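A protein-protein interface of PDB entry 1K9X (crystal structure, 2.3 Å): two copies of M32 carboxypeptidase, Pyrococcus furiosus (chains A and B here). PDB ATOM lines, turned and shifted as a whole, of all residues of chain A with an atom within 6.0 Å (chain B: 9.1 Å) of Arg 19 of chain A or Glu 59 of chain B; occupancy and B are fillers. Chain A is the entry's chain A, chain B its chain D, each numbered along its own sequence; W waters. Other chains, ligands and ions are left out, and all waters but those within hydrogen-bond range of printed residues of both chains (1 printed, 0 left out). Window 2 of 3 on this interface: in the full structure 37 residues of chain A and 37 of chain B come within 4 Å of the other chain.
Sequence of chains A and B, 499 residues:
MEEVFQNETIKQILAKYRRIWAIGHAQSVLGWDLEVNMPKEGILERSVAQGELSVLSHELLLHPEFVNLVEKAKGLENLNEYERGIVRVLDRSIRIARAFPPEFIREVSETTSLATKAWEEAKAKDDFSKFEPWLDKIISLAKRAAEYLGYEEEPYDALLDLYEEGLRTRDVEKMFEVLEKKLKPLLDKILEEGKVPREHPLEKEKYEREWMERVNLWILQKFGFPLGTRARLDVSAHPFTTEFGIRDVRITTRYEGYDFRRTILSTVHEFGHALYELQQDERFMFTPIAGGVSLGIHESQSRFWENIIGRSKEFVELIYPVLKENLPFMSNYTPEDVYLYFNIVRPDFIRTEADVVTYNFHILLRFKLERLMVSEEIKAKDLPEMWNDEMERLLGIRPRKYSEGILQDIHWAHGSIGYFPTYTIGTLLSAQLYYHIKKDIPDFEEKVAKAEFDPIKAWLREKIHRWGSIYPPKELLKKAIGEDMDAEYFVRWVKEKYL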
ATOM      1  N   LEU A  14     -15.926 -18.799 -14.836  1.00  0.00           N
ATOM      2  CA  LEU A  14     -15.246 -18.106 -15.923  1.00  0.00           C
ATOM      3  C   LEU A  14     -13.909 -18.750 -16.318  1.00  0.00           C
ATOM      4  O   LEU A  14     -13.588 -18.850 -17.505  1.00  0.00           O
ATOM      5  CB  LEU A  14     -15.023 -16.638 -15.542  1.00  0.00           C
ATOM      6  CG  LEU A  14     -16.306 -15.824 -15.303  1.00  0.00           C
ATOM      7  CD1 LEU A  14     -15.949 -14.383 -14.968  1.00  0.00           C
ATOM      8  CD2 LEU A  14     -17.187 -15.878 -16.544  1.00  0.00           C
ATOM      9  N   ALA A  15     -13.123 -19.177 -15.336  1.00  0.00           N
ATOM     10  CA  ALA A  15     -11.844 -19.821 -15.630  1.00  0.00           C
ATOM     11  C   ALA A  15     -12.070 -21.034 -16.539  1.00  0.00           C
ATOM     12  O   ALA A  15     -11.347 -21.243 -17.513  1.00  0.00           O
ATOM     13  CB  ALA A  15     -11.161 -20.258 -14.336  1.00  0.00           C
ATOM     14  N   LYS A  16     -13.079 -21.833 -16.210  1.00  0.00           N
ATOM     15  CA  LYS A  16     -13.407 -23.014 -17.002  1.00  0.00           C
ATOM     16  C   LYS A  16     -14.002 -22.638 -18.360  1.00  0.00           C
ATOM     17  O   LYS A  16     -13.730 -23.287 -19.376  1.00  0.00           O
ATOM     18  CB  LYS A  16     -14.398 -23.904 -16.237  1.00  0.00           C
ATOM     19  CG  LYS A  16     -13.759 -24.676 -15.100  1.00  0.00           C
ATOM     20  CD  LYS A  16     -14.756 -25.585 -14.403  1.00  0.00           C
ATOM     21  CE  LYS A  16     -14.085 -26.406 -13.302  1.00  0.00           C
ATOM     22  NZ  LYS A  16     -13.243 -27.515 -13.840  1.00  0.00           N
ATOM     23  N   TYR A  17     -14.801 -21.580 -18.379  1.00  0.00           N
ATOM     24  CA  TYR A  17     -15.444 -21.163 -19.611  1.00  0.00           C
ATOM     25  C   TYR A  17     -14.462 -20.745 -20.702  1.00  0.00           C
ATOM     26  O   TYR A  17     -14.763 -20.884 -21.893  1.00  0.00           O
ATOM     27  CB  TYR A  17     -16.419 -20.019 -19.341  1.00  0.00           C
ATOM     28  CG  TYR A  17     -17.309 -19.729 -20.526  1.00  0.00           C
ATOM     29  CD1 TYR A  17     -18.413 -20.528 -20.803  1.00  0.00           C
ATOM     30  CD2 TYR A  17     -17.024 -18.670 -21.391  1.00  0.00           C
ATOM     31  CE1 TYR A  17     -19.214 -20.282 -21.915  1.00  0.00           C
ATOM     32  CE2 TYR A  17     -17.812 -18.415 -22.501  1.00  0.00           C
ATOM     33  CZ  TYR A  17     -18.905 -19.222 -22.761  1.00  0.00           C
ATOM     34  OH  TYR A  17     -19.685 -18.970 -23.870  1.00  0.00           O
ATOM     35  N   ARG A  18     -13.297 -20.233 -20.309  1.00  0.00           N
ATOM     36  CA  ARG A  18     -12.307 -19.809 -21.297  1.00  0.00           C
ATOM     37  C   ARG A  18     -11.974 -20.938 -22.262  1.00  0.00           C
ATOM     38  O   ARG A  18     -11.681 -20.698 -23.426  1.00  0.00           O
ATOM     39  CB  ARG A  18     -11.022 -19.315 -20.622  1.00  0.00           C
ATOM     40  CG  ARG A  18     -11.106 -17.888 -20.090  1.00  0.00           C
ATOM     41  CD  ARG A  18      -9.726 -17.237 -20.028  1.00  0.00           C
ATOM     42  NE  ARG A  18      -9.780 -15.843 -19.595  1.00  0.00           N
ATOM     43  CZ  ARG A  18      -8.756 -14.993 -19.668  1.00  0.00           C
ATOM     44  NH1 ARG A  18      -7.591 -15.395 -20.165  1.00  0.00           N
ATOM     45  NH2 ARG A  18      -8.896 -13.741 -19.234  1.00  0.00           N
ATOM     46  N   ARG A  19     -12.016 -22.170 -21.772  1.00  0.00           N
ATOM     47  CA  ARG A  19     -11.730 -23.318 -22.617  1.00  0.00           C
ATOM     48  C   ARG A  19     -12.852 -23.385 -23.649  1.00  0.00           C
ATOM     49  O   ARG A  19     -12.604 -23.451 -24.852  1.00  0.00           O
ATOM     50  CB  ARG A  19     -11.696 -24.595 -21.772  1.00  0.00           C
ATOM     51  CG  ARG A  19     -11.111 -25.819 -22.468  1.00  0.00           C
ATOM     52  CD  ARG A  19     -11.090 -27.015 -21.510  1.00  0.00           C
ATOM     53  NE  ARG A  19      -9.757 -27.573 -21.259  1.00  0.00           N
ATOM     54  CZ  ARG A  19      -8.664 -26.859 -20.992  1.00  0.00           C
ATOM     55  NH1 ARG A  19      -8.706 -25.530 -20.946  1.00  0.00           N
ATOM     56  NH2 ARG A  19      -7.521 -27.482 -20.741  1.00  0.00           N
ATOM     57  N   ILE A  20     -14.091 -23.355 -23.168  1.00  0.00           N
ATOM     58  CA  ILE A  20     -15.253 -23.400 -24.045  1.00  0.00           C
ATOM     59  C   ILE A  20     -15.193 -22.207 -24.990  1.00  0.00           C
ATOM     60  O   ILE A  20     -15.362 -22.348 -26.196  1.00  0.00           O
ATOM     61  CB  ILE A  20     -16.563 -23.360 -23.225  1.00  0.00           C
ATOM     62  CG1 ILE A  20     -16.586 -24.533 -22.243  1.00  0.00           C
ATOM     63  CG2 ILE A  20     -17.767 -23.430 -24.149  1.00  0.00           C
ATOM     64  CD1 ILE A  20     -17.865 -24.659 -21.423  1.00  0.00           C
ATOM     65  N   TRP A  21     -14.926 -21.029 -24.441  1.00  0.00           N
ATOM     66  CA  TRP A  21     -14.833 -19.836 -25.263  1.00  0.00           C
ATOM     67  C   TRP A  21     -13.795 -20.027 -26.362  1.00  0.00           C
ATOM     68  O   TRP A  21     -14.031 -19.651 -27.508  1.00  0.00           O
ATOM     69  CB  TRP A  21     -14.440 -18.622 -24.429  1.00  0.00           C
ATOM     70  CG  TRP A  21     -14.202 -17.407 -25.282  1.00  0.00           C
ATOM     71  CD1 TRP A  21     -15.130 -16.485 -25.685  1.00  0.00           C
ATOM     72  CD2 TRP A  21     -12.969 -17.034 -25.906  1.00  0.00           C
ATOM     73  NE1 TRP A  21     -14.548 -15.565 -26.525  1.00  0.00           N
ATOM     74  CE2 TRP A  21     -13.224 -15.879 -26.679  1.00  0.00           C
ATOM     75  CE3 TRP A  21     -11.670 -17.567 -25.888  1.00  0.00           C
ATOM     76  CZ2 TRP A  21     -12.227 -15.245 -27.431  1.00  0.00           C
ATOM     77  CZ3 TRP A  21     -10.681 -16.941 -26.631  1.00  0.00           C
ATOM     78  CH2 TRP A  21     -10.969 -15.788 -27.396  1.00  0.00           C
ATOM     79  N   ALA A  22     -12.645 -20.603 -26.004  1.00  0.00           N
ATOM     80  CA  ALA A  22     -11.562 -20.826 -26.967  1.00  0.00           C
ATOM     81  C   ALA A  22     -11.979 -21.693 -28.172  1.00  0.00           C
ATOM     82  O   ALA A  22     -11.592 -21.426 -29.307  1.00  0.00           O
ATOM     83  CB  ALA A  22     -10.373 -21.454 -26.265  1.00  0.00           C
ATOM     84  N   ILE A  23     -12.769 -22.730 -27.919  1.00  0.00           N
ATOM     85  CA  ILE A  23     -13.232 -23.609 -28.987  1.00  0.00           C
ATOM     86  C   ILE A  23     -14.177 -22.873 -29.938  1.00  0.00           C
ATOM     87  O   ILE A  23     -14.166 -23.104 -31.160  1.00  0.00           O
ATOM     88  CB  ILE A  23     -13.914 -24.854 -28.388  1.00  0.00           C
ATOM     89  CG1 ILE A  23     -12.876 -25.631 -27.575  1.00  0.00           C
ATOM     90  CG2 ILE A  23     -14.503 -25.732 -29.501  1.00  0.00           C
ATOM     91  CD1 ILE A  23     -13.416 -26.833 -26.856  1.00  0.00           C
ATOM     92  N   GLY A  24     -14.982 -21.974 -29.373  1.00  0.00           N
ATOM     93  CA  GLY A  24     -15.909 -21.192 -30.172  1.00  0.00           C
ATOM     94  C   GLY A  24     -15.129 -20.252 -31.065  1.00  0.00           C
ATOM     95  O   GLY A  24     -15.513 -19.973 -32.202  1.00  0.00           O
ATOM     96  N   LEU A  60     -17.751 -30.188 -22.585  1.00  0.00           N
ATOM     97  CA  LEU A  60     -17.256 -29.287 -21.543  1.00  0.00           C
ATOM     98  C   LEU A  60     -18.392 -28.501 -20.892  1.00  0.00           C
ATOM     99  O   LEU A  60     -18.342 -28.195 -19.695  1.00  0.00           O
ATOM    100  CB  LEU A  60     -16.239 -28.297 -22.117  1.00  0.00           C
ATOM    101  CG  LEU A  60     -14.949 -28.863 -22.715  1.00  0.00           C
ATOM    102  CD1 LEU A  60     -14.023 -27.713 -23.106  1.00  0.00           C
ATOM    103  CD2 LEU A  60     -14.264 -29.770 -21.702  1.00  0.00           C
ATOM    104  N   ARG B  19      -9.785 -36.218 -31.807  1.00  0.00           N
ATOM    105  CA  ARG B  19     -10.023 -35.001 -31.042  1.00  0.00           C
ATOM    106  C   ARG B  19      -8.729 -34.191 -31.009  1.00  0.00           C
ATOM    107  O   ARG B  19      -8.746 -32.971 -31.168  1.00  0.00           O
ATOM    108  CB  ARG B  19     -10.460 -35.315 -29.609  1.00  0.00           C
ATOM    109  CG  ARG B  19     -10.720 -34.060 -28.806  1.00  0.00           C
ATOM    110  CD  ARG B  19     -10.972 -34.290 -27.322  1.00  0.00           C
ATOM    111  NE  ARG B  19     -12.212 -34.997 -26.998  1.00  0.00           N
ATOM    112  CZ  ARG B  19     -13.375 -34.845 -27.626  1.00  0.00           C
ATOM    113  NH1 ARG B  19     -13.493 -34.008 -28.649  1.00  0.00           N
ATOM    114  NH2 ARG B  19     -14.437 -35.519 -27.207  1.00  0.00           N
ATOM    115  N   ILE B  20      -7.611 -34.883 -30.800  1.00  0.00           N
ATOM    116  CA  ILE B  20      -6.292 -34.244 -30.764  1.00  0.00           C
ATOM    117  C   ILE B  20      -5.980 -33.696 -32.154  1.00  0.00           C
ATOM    118  O   ILE B  20      -5.497 -32.577 -32.299  1.00  0.00           O
ATOM    119  CB  ILE B  20      -5.185 -35.251 -30.339  1.00  0.00           C
ATOM    120  CG1 ILE B  20      -5.415 -35.682 -28.885  1.00  0.00           C
ATOM    121  CG2 ILE B  20      -3.802 -34.629 -30.506  1.00  0.00           C
ATOM    122  CD1 ILE B  20      -4.399 -36.664 -28.351  1.00  0.00           C
ATOM    123  N   ILE B  23      -8.041 -30.519 -32.817  1.00  0.00           N
ATOM    124  CA  ILE B  23      -7.489 -29.353 -32.156  1.00  0.00           C
ATOM    125  C   ILE B  23      -6.276 -28.837 -32.933  1.00  0.00           C
ATOM    126  O   ILE B  23      -6.055 -27.630 -33.000  1.00  0.00           O
ATOM    127  CB  ILE B  23      -7.130 -29.682 -30.692  1.00  0.00           C
ATOM    128  CG1 ILE B  23      -8.412 -30.083 -29.946  1.00  0.00           C
ATOM    129  CG2 ILE B  23      -6.461 -28.474 -30.020  1.00  0.00           C
ATOM    130  CD1 ILE B  23      -8.207 -30.469 -28.484  1.00  0.00           C
ATOM    131  N   VAL B  48      -5.081 -15.895 -26.440  1.00  0.00           N
ATOM    132  CA  VAL B  48      -5.611 -16.707 -25.349  1.00  0.00           C
ATOM    133  C   VAL B  48      -6.250 -17.984 -25.888  1.00  0.00           C
ATOM    134  O   VAL B  48      -6.166 -19.033 -25.246  1.00  0.00           O
ATOM    135  CB  VAL B  48      -6.664 -15.949 -24.482  1.00  0.00           C
ATOM    136  CG1 VAL B  48      -6.101 -14.617 -24.005  1.00  0.00           C
ATOM    137  CG2 VAL B  48      -7.935 -15.749 -25.259  1.00  0.00           C
ATOM    138  N   ALA B  49      -6.888 -17.896 -27.060  1.00  0.00           N
ATOM    139  CA  ALA B  49      -7.532 -19.066 -27.666  1.00  0.00           C
ATOM    140  C   ALA B  49      -6.463 -20.112 -27.973  1.00  0.00           C
ATOM    141  O   ALA B  49      -6.636 -21.291 -27.674  1.00  0.00           O
ATOM    142  CB  ALA B  49      -8.269 -18.676 -28.938  1.00  0.00           C
ATOM    143  N   GLN B  50      -5.360 -19.673 -28.573  1.00  0.00           N
ATOM    144  CA  GLN B  50      -4.256 -20.577 -28.892  1.00  0.00           C
ATOM    145  C   GLN B  50      -3.707 -21.197 -27.610  1.00  0.00           C
ATOM    146  O   GLN B  50      -3.499 -22.404 -27.541  1.00  0.00           O
ATOM    147  CB  GLN B  50      -3.140 -19.820 -29.618  1.00  0.00           C
ATOM    148  CG  GLN B  50      -3.506 -19.411 -31.032  1.00  0.00           C
ATOM    149  CD  GLN B  50      -2.504 -18.452 -31.641  1.00  0.00           C
ATOM    150  OE1 GLN B  50      -2.259 -17.372 -31.107  1.00  0.00           O
ATOM    151  NE2 GLN B  50      -1.926 -18.840 -32.767  1.00  0.00           N
ATOM    152  N   GLY B  51      -3.466 -20.368 -26.595  1.00  0.00           N
ATOM    153  CA  GLY B  51      -2.953 -20.889 -25.338  1.00  0.00           C
ATOM    154  C   GLY B  51      -3.853 -21.990 -24.792  1.00  0.00           C
ATOM    155  O   GLY B  51      -3.394 -23.106 -24.507  1.00  0.00           O
ATOM    156  N   GLU B  52      -5.139 -21.673 -24.642  1.00  0.00           N
ATOM    157  CA  GLU B  52      -6.121 -22.635 -24.145  1.00  0.00           C
ATOM    158  C   GLU B  52      -6.080 -23.933 -24.954  1.00  0.00           C
ATOM    159  O   GLU B  52      -6.035 -25.021 -24.384  1.00  0.00           O
ATOM    160  CB  GLU B  52      -7.528 -22.044 -24.226  1.00  0.00           C
ATOM    161  CG  GLU B  52      -7.779 -20.854 -23.329  1.00  0.00           C
ATOM    162  CD  GLU B  52      -7.795 -21.228 -21.864  1.00  0.00           C
ATOM    163  OE1 GLU B  52      -8.226 -22.355 -21.537  1.00  0.00           O
ATOM    164  OE2 GLU B  52      -7.395 -20.386 -21.035  1.00  0.00           O
ATOM    165  N   LEU B  53      -6.098 -23.817 -26.279  1.00  0.00           N
ATOM    166  CA  LEU B  53      -6.046 -24.995 -27.142  1.00  0.00           C
ATOM    167  C   LEU B  53      -4.776 -25.812 -26.900  1.00  0.00           C
ATOM    168  O   LEU B  53      -4.844 -27.039 -26.823  1.00  0.00           O
ATOM    169  CB  LEU B  53      -6.129 -24.593 -28.615  1.00  0.00           C
ATOM    170  CG  LEU B  53      -7.425 -23.925 -29.091  1.00  0.00           C
ATOM    171  CD1 LEU B  53      -7.356 -23.708 -30.589  1.00  0.00           C
ATOM    172  CD2 LEU B  53      -8.617 -24.789 -28.756  1.00  0.00           C
ATOM    173  N   SER B  54      -3.625 -25.143 -26.778  1.00  0.00           N
ATOM    174  CA  SER B  54      -2.356 -25.843 -26.525  1.00  0.00           C
ATOM    175  C   SER B  54      -2.434 -26.671 -25.246  1.00  0.00           C
ATOM    176  O   SER B  54      -2.026 -27.828 -25.228  1.00  0.00           O
ATOM    177  CB  SER B  54      -1.178 -24.859 -26.392  1.00  0.00           C
ATOM    178  OG  SER B  54      -0.695 -24.431 -27.653  1.00  0.00           O
ATOM    179  N   VAL B  55      -2.949 -26.072 -24.176  1.00  0.00           N
ATOM    180  CA  VAL B  55      -3.066 -26.781 -22.913  1.00  0.00           C
ATOM    181  C   VAL B  55      -4.032 -27.944 -23.048  1.00  0.00           C
ATOM    182  O   VAL B  55      -3.801 -29.022 -22.489  1.00  0.00           O
ATOM    183  CB  VAL B  55      -3.567 -25.864 -21.762  1.00  0.00           C
ATOM    184  CG1 VAL B  55      -3.802 -26.701 -20.507  1.00  0.00           C
ATOM    185  CG2 VAL B  55      -2.547 -24.758 -21.476  1.00  0.00           C
ATOM    186  N   LEU B  56      -5.113 -27.737 -23.787  1.00  0.00           N
ATOM    187  CA  LEU B  56      -6.090 -28.802 -23.965  1.00  0.00           C
ATOM    188  C   LEU B  56      -5.443 -30.000 -24.659  1.00  0.00           C
ATOM    189  O   LEU B  56      -5.512 -31.123 -24.162  1.00  0.00           O
ATOM    190  CB  LEU B  56      -7.279 -28.316 -24.802  1.00  0.00           C
ATOM    191  CG  LEU B  56      -8.688 -28.842 -24.498  1.00  0.00           C
ATOM    192  CD1 LEU B  56      -9.554 -28.639 -25.726  1.00  0.00           C
ATOM    193  CD2 LEU B  56      -8.671 -30.307 -24.120  1.00  0.00           C
ATOM    194  N   SER B  57      -4.805 -29.764 -25.799  1.00  0.00           N
ATOM    195  CA  SER B  57      -4.188 -30.862 -26.537  1.00  0.00           C
ATOM    196  C   SER B  57      -3.152 -31.621 -25.724  1.00  0.00           C
ATOM    197  O   SER B  57      -3.075 -32.842 -25.810  1.00  0.00           O
ATOM    198  CB  SER B  57      -3.579 -30.359 -27.853  1.00  0.00           C
ATOM    199  OG  SER B  57      -2.857 -29.159 -27.663  1.00  0.00           O
ATOM    200  N   HIS B  58      -2.359 -30.912 -24.929  1.00  0.00           N
ATOM    201  CA  HIS B  58      -1.349 -31.569 -24.104  1.00  0.00           C
ATOM    202  C   HIS B  58      -2.056 -32.483 -23.104  1.00  0.00           C
ATOM    203  O   HIS B  58      -1.664 -33.631 -22.890  1.00  0.00           O
ATOM    204  CB  HIS B  58      -0.521 -30.523 -23.350  1.00  0.00           C
ATOM    205  CG  HIS B  58       0.622 -31.103 -22.580  1.00  0.00           C
ATOM    206  ND1 HIS B  58       1.658 -31.779 -23.185  1.00  0.00           N
ATOM    207  CD2 HIS B  58       0.889 -31.114 -21.252  1.00  0.00           C
ATOM    208  CE1 HIS B  58       2.516 -32.181 -22.263  1.00  0.00           C
ATOM    209  NE2 HIS B  58       2.071 -31.790 -21.082  1.00  0.00           N
ATOM    210  N   GLU B  59      -3.112 -31.950 -22.504  1.00  0.00           N
ATOM    211  CA  GLU B  59      -3.925 -32.665 -21.528  1.00  0.00           C
ATOM    212  C   GLU B  59      -4.396 -33.993 -22.121  1.00  0.00           C
ATOM    213  O   GLU B  59      -4.170 -35.065 -21.550  1.00  0.00           O
ATOM    214  CB  GLU B  59      -5.108 -31.780 -21.168  1.00  0.00           C
ATOM    215  CG  GLU B  59      -5.938 -32.206 -19.995  1.00  0.00           C
ATOM    216  CD  GLU B  59      -6.889 -31.096 -19.585  1.00  0.00           C
ATOM    217  OE1 GLU B  59      -6.393 -30.012 -19.193  1.00  0.00           O
ATOM    218  OE2 GLU B  59      -8.123 -31.302 -19.669  1.00  0.00           O
ATOM    219  N   LEU B  60      -5.044 -33.912 -23.278  1.00  0.00           N
ATOM    220  CA  LEU B  60      -5.537 -35.093 -23.978  1.00  0.00           C
ATOM    221  C   LEU B  60      -4.404 -36.086 -24.297  1.00  0.00           C
ATOM    222  O   LEU B  60      -4.549 -37.300 -24.124  1.00  0.00           O
ATOM    223  CB  LEU B  60      -6.229 -34.661 -25.265  1.00  0.00           C
ATOM    224  CG  LEU B  60      -7.439 -33.745 -25.035  1.00  0.00           C
ATOM    225  CD1 LEU B  60      -7.881 -33.134 -26.343  1.00  0.00           C
ATOM    226  CD2 LEU B  60      -8.573 -34.547 -24.392  1.00  0.00           C
ATOM    227  N   LEU B  61      -3.273 -35.572 -24.760  1.00  0.00           N
ATOM    228  CA  LEU B  61      -2.155 -36.437 -25.088  1.00  0.00           C
ATOM    229  C   LEU B  61      -1.672 -37.237 -23.874  1.00  0.00           C
ATOM    230  O   LEU B  61      -1.272 -38.381 -24.017  1.00  0.00           O
ATOM    231  CB  LEU B  61      -0.997 -35.612 -25.660  1.00  0.00           C
ATOM    232  CG  LEU B  61       0.207 -36.407 -26.168  1.00  0.00           C
ATOM    233  CD1 LEU B  61      -0.240 -37.324 -27.294  1.00  0.00           C
ATOM    234  CD2 LEU B  61       1.293 -35.446 -26.653  1.00  0.00           C
ATOM    235  N   LEU B  62      -1.711 -36.634 -22.685  1.00  0.00           N
ATOM    236  CA  LEU B  62      -1.271 -37.316 -21.463  1.00  0.00           C
ATOM    237  C   LEU B  62      -2.376 -37.931 -20.609  1.00  0.00           C
ATOM    238  O   LEU B  62      -2.109 -38.381 -19.496  1.00  0.00           O
ATOM    239  CB  LEU B  62      -0.448 -36.378 -20.571  1.00  0.00           C
ATOM    240  CG  LEU B  62       1.002 -36.110 -20.973  1.00  0.00           C
ATOM    241  CD1 LEU B  62       1.673 -37.427 -21.368  1.00  0.00           C
ATOM    242  CD2 LEU B  62       1.042 -35.145 -22.132  1.00  0.00           C
ATOM    243  N   HIS B  63      -3.608 -37.954 -21.108  1.00  0.00           N
ATOM    244  CA  HIS B  63      -4.697 -38.546 -20.337  1.00  0.00           C
ATOM    245  C   HIS B  63      -4.413 -40.028 -20.111  1.00  0.00           C
ATOM    246  O   HIS B  63      -4.142 -40.767 -21.060  1.00  0.00           O
ATOM    247  CB  HIS B  63      -6.030 -38.403 -21.065  1.00  0.00           C
ATOM    248  CG  HIS B  63      -7.204 -38.799 -20.228  1.00  0.00           C
ATOM    249  ND1 HIS B  63      -7.351 -40.065 -19.705  1.00  0.00           N
ATOM    250  CD2 HIS B  63      -8.264 -38.082 -19.782  1.00  0.00           C
ATOM    251  CE1 HIS B  63      -8.450 -40.113 -18.974  1.00  0.00           C
ATOM    252  NE2 HIS B  63      -9.022 -38.922 -19.005  1.00  0.00           N
ATOM    253  N   PRO B  64      -4.484 -40.486 -18.850  1.00  0.00           N
ATOM    254  CA  PRO B  64      -4.227 -41.887 -18.511  1.00  0.00           C
ATOM    255  C   PRO B  64      -4.896 -42.920 -19.416  1.00  0.00           C
ATOM    256  O   PRO B  64      -4.333 -43.984 -19.657  1.00  0.00           O
ATOM    257  CB  PRO B  64      -4.700 -41.979 -17.065  1.00  0.00           C
ATOM    258  CG  PRO B  64      -4.347 -40.622 -16.537  1.00  0.00           C
ATOM    259  CD  PRO B  64      -4.847 -39.723 -17.644  1.00  0.00           C
ATOM    260  N   GLU B  65      -6.086 -42.625 -19.919  1.00  0.00           N
ATOM    261  CA  GLU B  65      -6.755 -43.588 -20.787  1.00  0.00           C
ATOM    262  C   GLU B  65      -6.035 -43.699 -22.122  1.00  0.00           C
ATOM    263  O   GLU B  65      -5.843 -44.792 -22.643  1.00  0.00           O
ATOM    264  CB  GLU B  65      -8.210 -43.186 -21.029  1.00  0.00           C
ATOM    265  CG  GLU B  65      -9.137 -43.447 -19.857  1.00  0.00           C
ATOM    266  CD  GLU B  65     -10.566 -43.031 -20.150  1.00  0.00           C
ATOM    267  OE1 GLU B  65     -11.130 -43.520 -21.150  1.00  0.00           O
ATOM    268  OE2 GLU B  65     -11.127 -42.217 -19.384  1.00  0.00           O
ATOM    269  N   PHE B  66      -5.631 -42.560 -22.672  1.00  0.00           N
ATOM    270  CA  PHE B  66      -4.946 -42.552 -23.952  1.00  0.00           C
ATOM    271  C   PHE B  66      -3.554 -43.159 -23.842  1.00  0.00           C
ATOM    272  O   PHE B  66      -3.170 -43.990 -24.670  1.00  0.00           O
ATOM    273  CB  PHE B  66      -4.851 -41.129 -24.491  1.00  0.00           C
ATOM    274  CG  PHE B  66      -4.427 -41.058 -25.926  1.00  0.00           C
ATOM    275  CD1 PHE B  66      -5.269 -41.524 -26.936  1.00  0.00           C
ATOM    276  CD2 PHE B  66      -3.180 -40.552 -26.270  1.00  0.00           C
ATOM    277  CE1 PHE B  66      -4.873 -41.486 -28.276  1.00  0.00           C
ATOM    278  CE2 PHE B  66      -2.769 -40.508 -27.601  1.00  0.00           C
ATOM    279  CZ  PHE B  66      -3.617 -40.977 -28.612  1.00  0.00           C
ATOM    280  N   VAL B  67      -2.793 -42.761 -22.826  1.00  0.00           N
ATOM    281  CA  VAL B  67      -1.455 -43.310 -22.684  1.00  0.00           C
ATOM    282  C   VAL B  67      -1.524 -44.817 -22.481  1.00  0.00           C
ATOM    283  O   VAL B  67      -0.770 -45.559 -23.116  1.00  0.00           O
ATOM    284  CB  VAL B  67      -0.664 -42.668 -21.506  1.00  0.00           C
ATOM    285  CG1 VAL B  67      -0.602 -41.160 -21.676  1.00  0.00           C
ATOM    286  CG2 VAL B  67      -1.294 -43.043 -20.184  1.00  0.00           C
ATOM    287  N   ILE B  94       4.329 -39.002 -26.485  1.00  0.00           N
ATOM    288  CA  ILE B  94       3.959 -39.106 -25.085  1.00  0.00           C
ATOM    289  C   ILE B  94       5.182 -39.022 -24.180  1.00  0.00           C
ATOM    290  O   ILE B  94       5.145 -38.367 -23.142  1.00  0.00           O
ATOM    291  CB  ILE B  94       3.186 -40.426 -24.807  1.00  0.00           C
ATOM    292  CG1 ILE B  94       1.859 -40.422 -25.586  1.00  0.00           C
ATOM    293  CG2 ILE B  94       2.932 -40.583 -23.301  1.00  0.00           C
ATOM    294  CD1 ILE B  94       0.999 -41.654 -25.380  1.00  0.00           C
ATOM    295  N   ALA B  97       6.341 -35.346 -24.272  1.00  0.00           N
ATOM    296  CA  ALA B  97       5.331 -34.523 -23.624  1.00  0.00           C
ATOM    297  C   ALA B  97       5.323 -34.669 -22.103  1.00  0.00           C
ATOM    298  O   ALA B  97       4.820 -33.792 -21.403  1.00  0.00           O
ATOM    299  CB  ALA B  97       3.954 -34.859 -24.180  1.00  0.00           C
HETATM  300  O   HOH W   1      -6.465 -18.188 -20.584  1.00  0.00           O
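Water W1 bridges the side-chain carboxylate (OE2) of Glu 52 of chain B (2.4 Å) and the guanidinium group (NH1) of Arg 18 of chain A (3.0 Å).
4 positions are printed for both chains.
Among the printed residues, merely in contact across the chains: Arg 18 of chain A with Glu 52 of chain B, Arg 19 of chain A with Val 55 of chain B, Arg 19 of chain A with Leu 56 of chain B, Trp 21 of chain A with Val 48 of chain B, Trp 21 of chain A with Ala 49 of chain B, Ala 22 of chain A with Ala 49 of chain B and Ala 22 of chain A with Glu 52 of chain B.
Arg 19 of chain A touches just these residues of chain B: Glu 52, Val 55, Leu 56 and Glu 59.
Glu 59 of chain B touches just one residue of chain A: Arg 19 (3.2 Å).
Of chain B, only Ala 49 and Glu 52 come within 4 Å of Ala 22 of chain A.
Printed residues of chain B within 4 Å of Trp 21 of chain A: Val 48 and Ala 49.
Printed residues of chain A within 4 Å of Leu 56 of chain B: Arg 19 (3.6 Å).
Printed residues of chain A within 4 Å of Ala 49 of chain B: Trp 21 (3.8 Å) and Ala 22 (3.97 Å).
Printed residues of chain B within 4 Å of Arg 18 of chain A: Glu 52.
Printed residues of chain A that touch a printed residue of chain B: Arg 18, Arg 19, Trp 21 and Ala 22.
Printed residues of chain B that touch a printed residue of chain A: Val 48, Ala 49, Glu 52, Val 55, Leu 56 and Glu 59.
Hydrophobic or aromatic side chains of chain B within 4 Å of the printed part of chain A: Val 48, Ala 49, Val 55 and Leu 56.
Among the printed residues, 9 pairs touch across the chains.
Among the printed residues, Asp or Glu carboxylates within 4 Å of a Lys or Arg side-chain nitrogen of the other chain: Arg 19 of chain A with Glu 52 of chain B and Arg 19 of chain A with Glu 59 of chain B.
NH2 of Arg 19 of chain A lies within salt-bridge range of OE1 of Glu 59 of chain B, at 3.2 Å.
NH1 of Arg 19 of chain A lies within salt-bridge range of OE1 of Glu 52 of chain B, 3.3 Å away.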
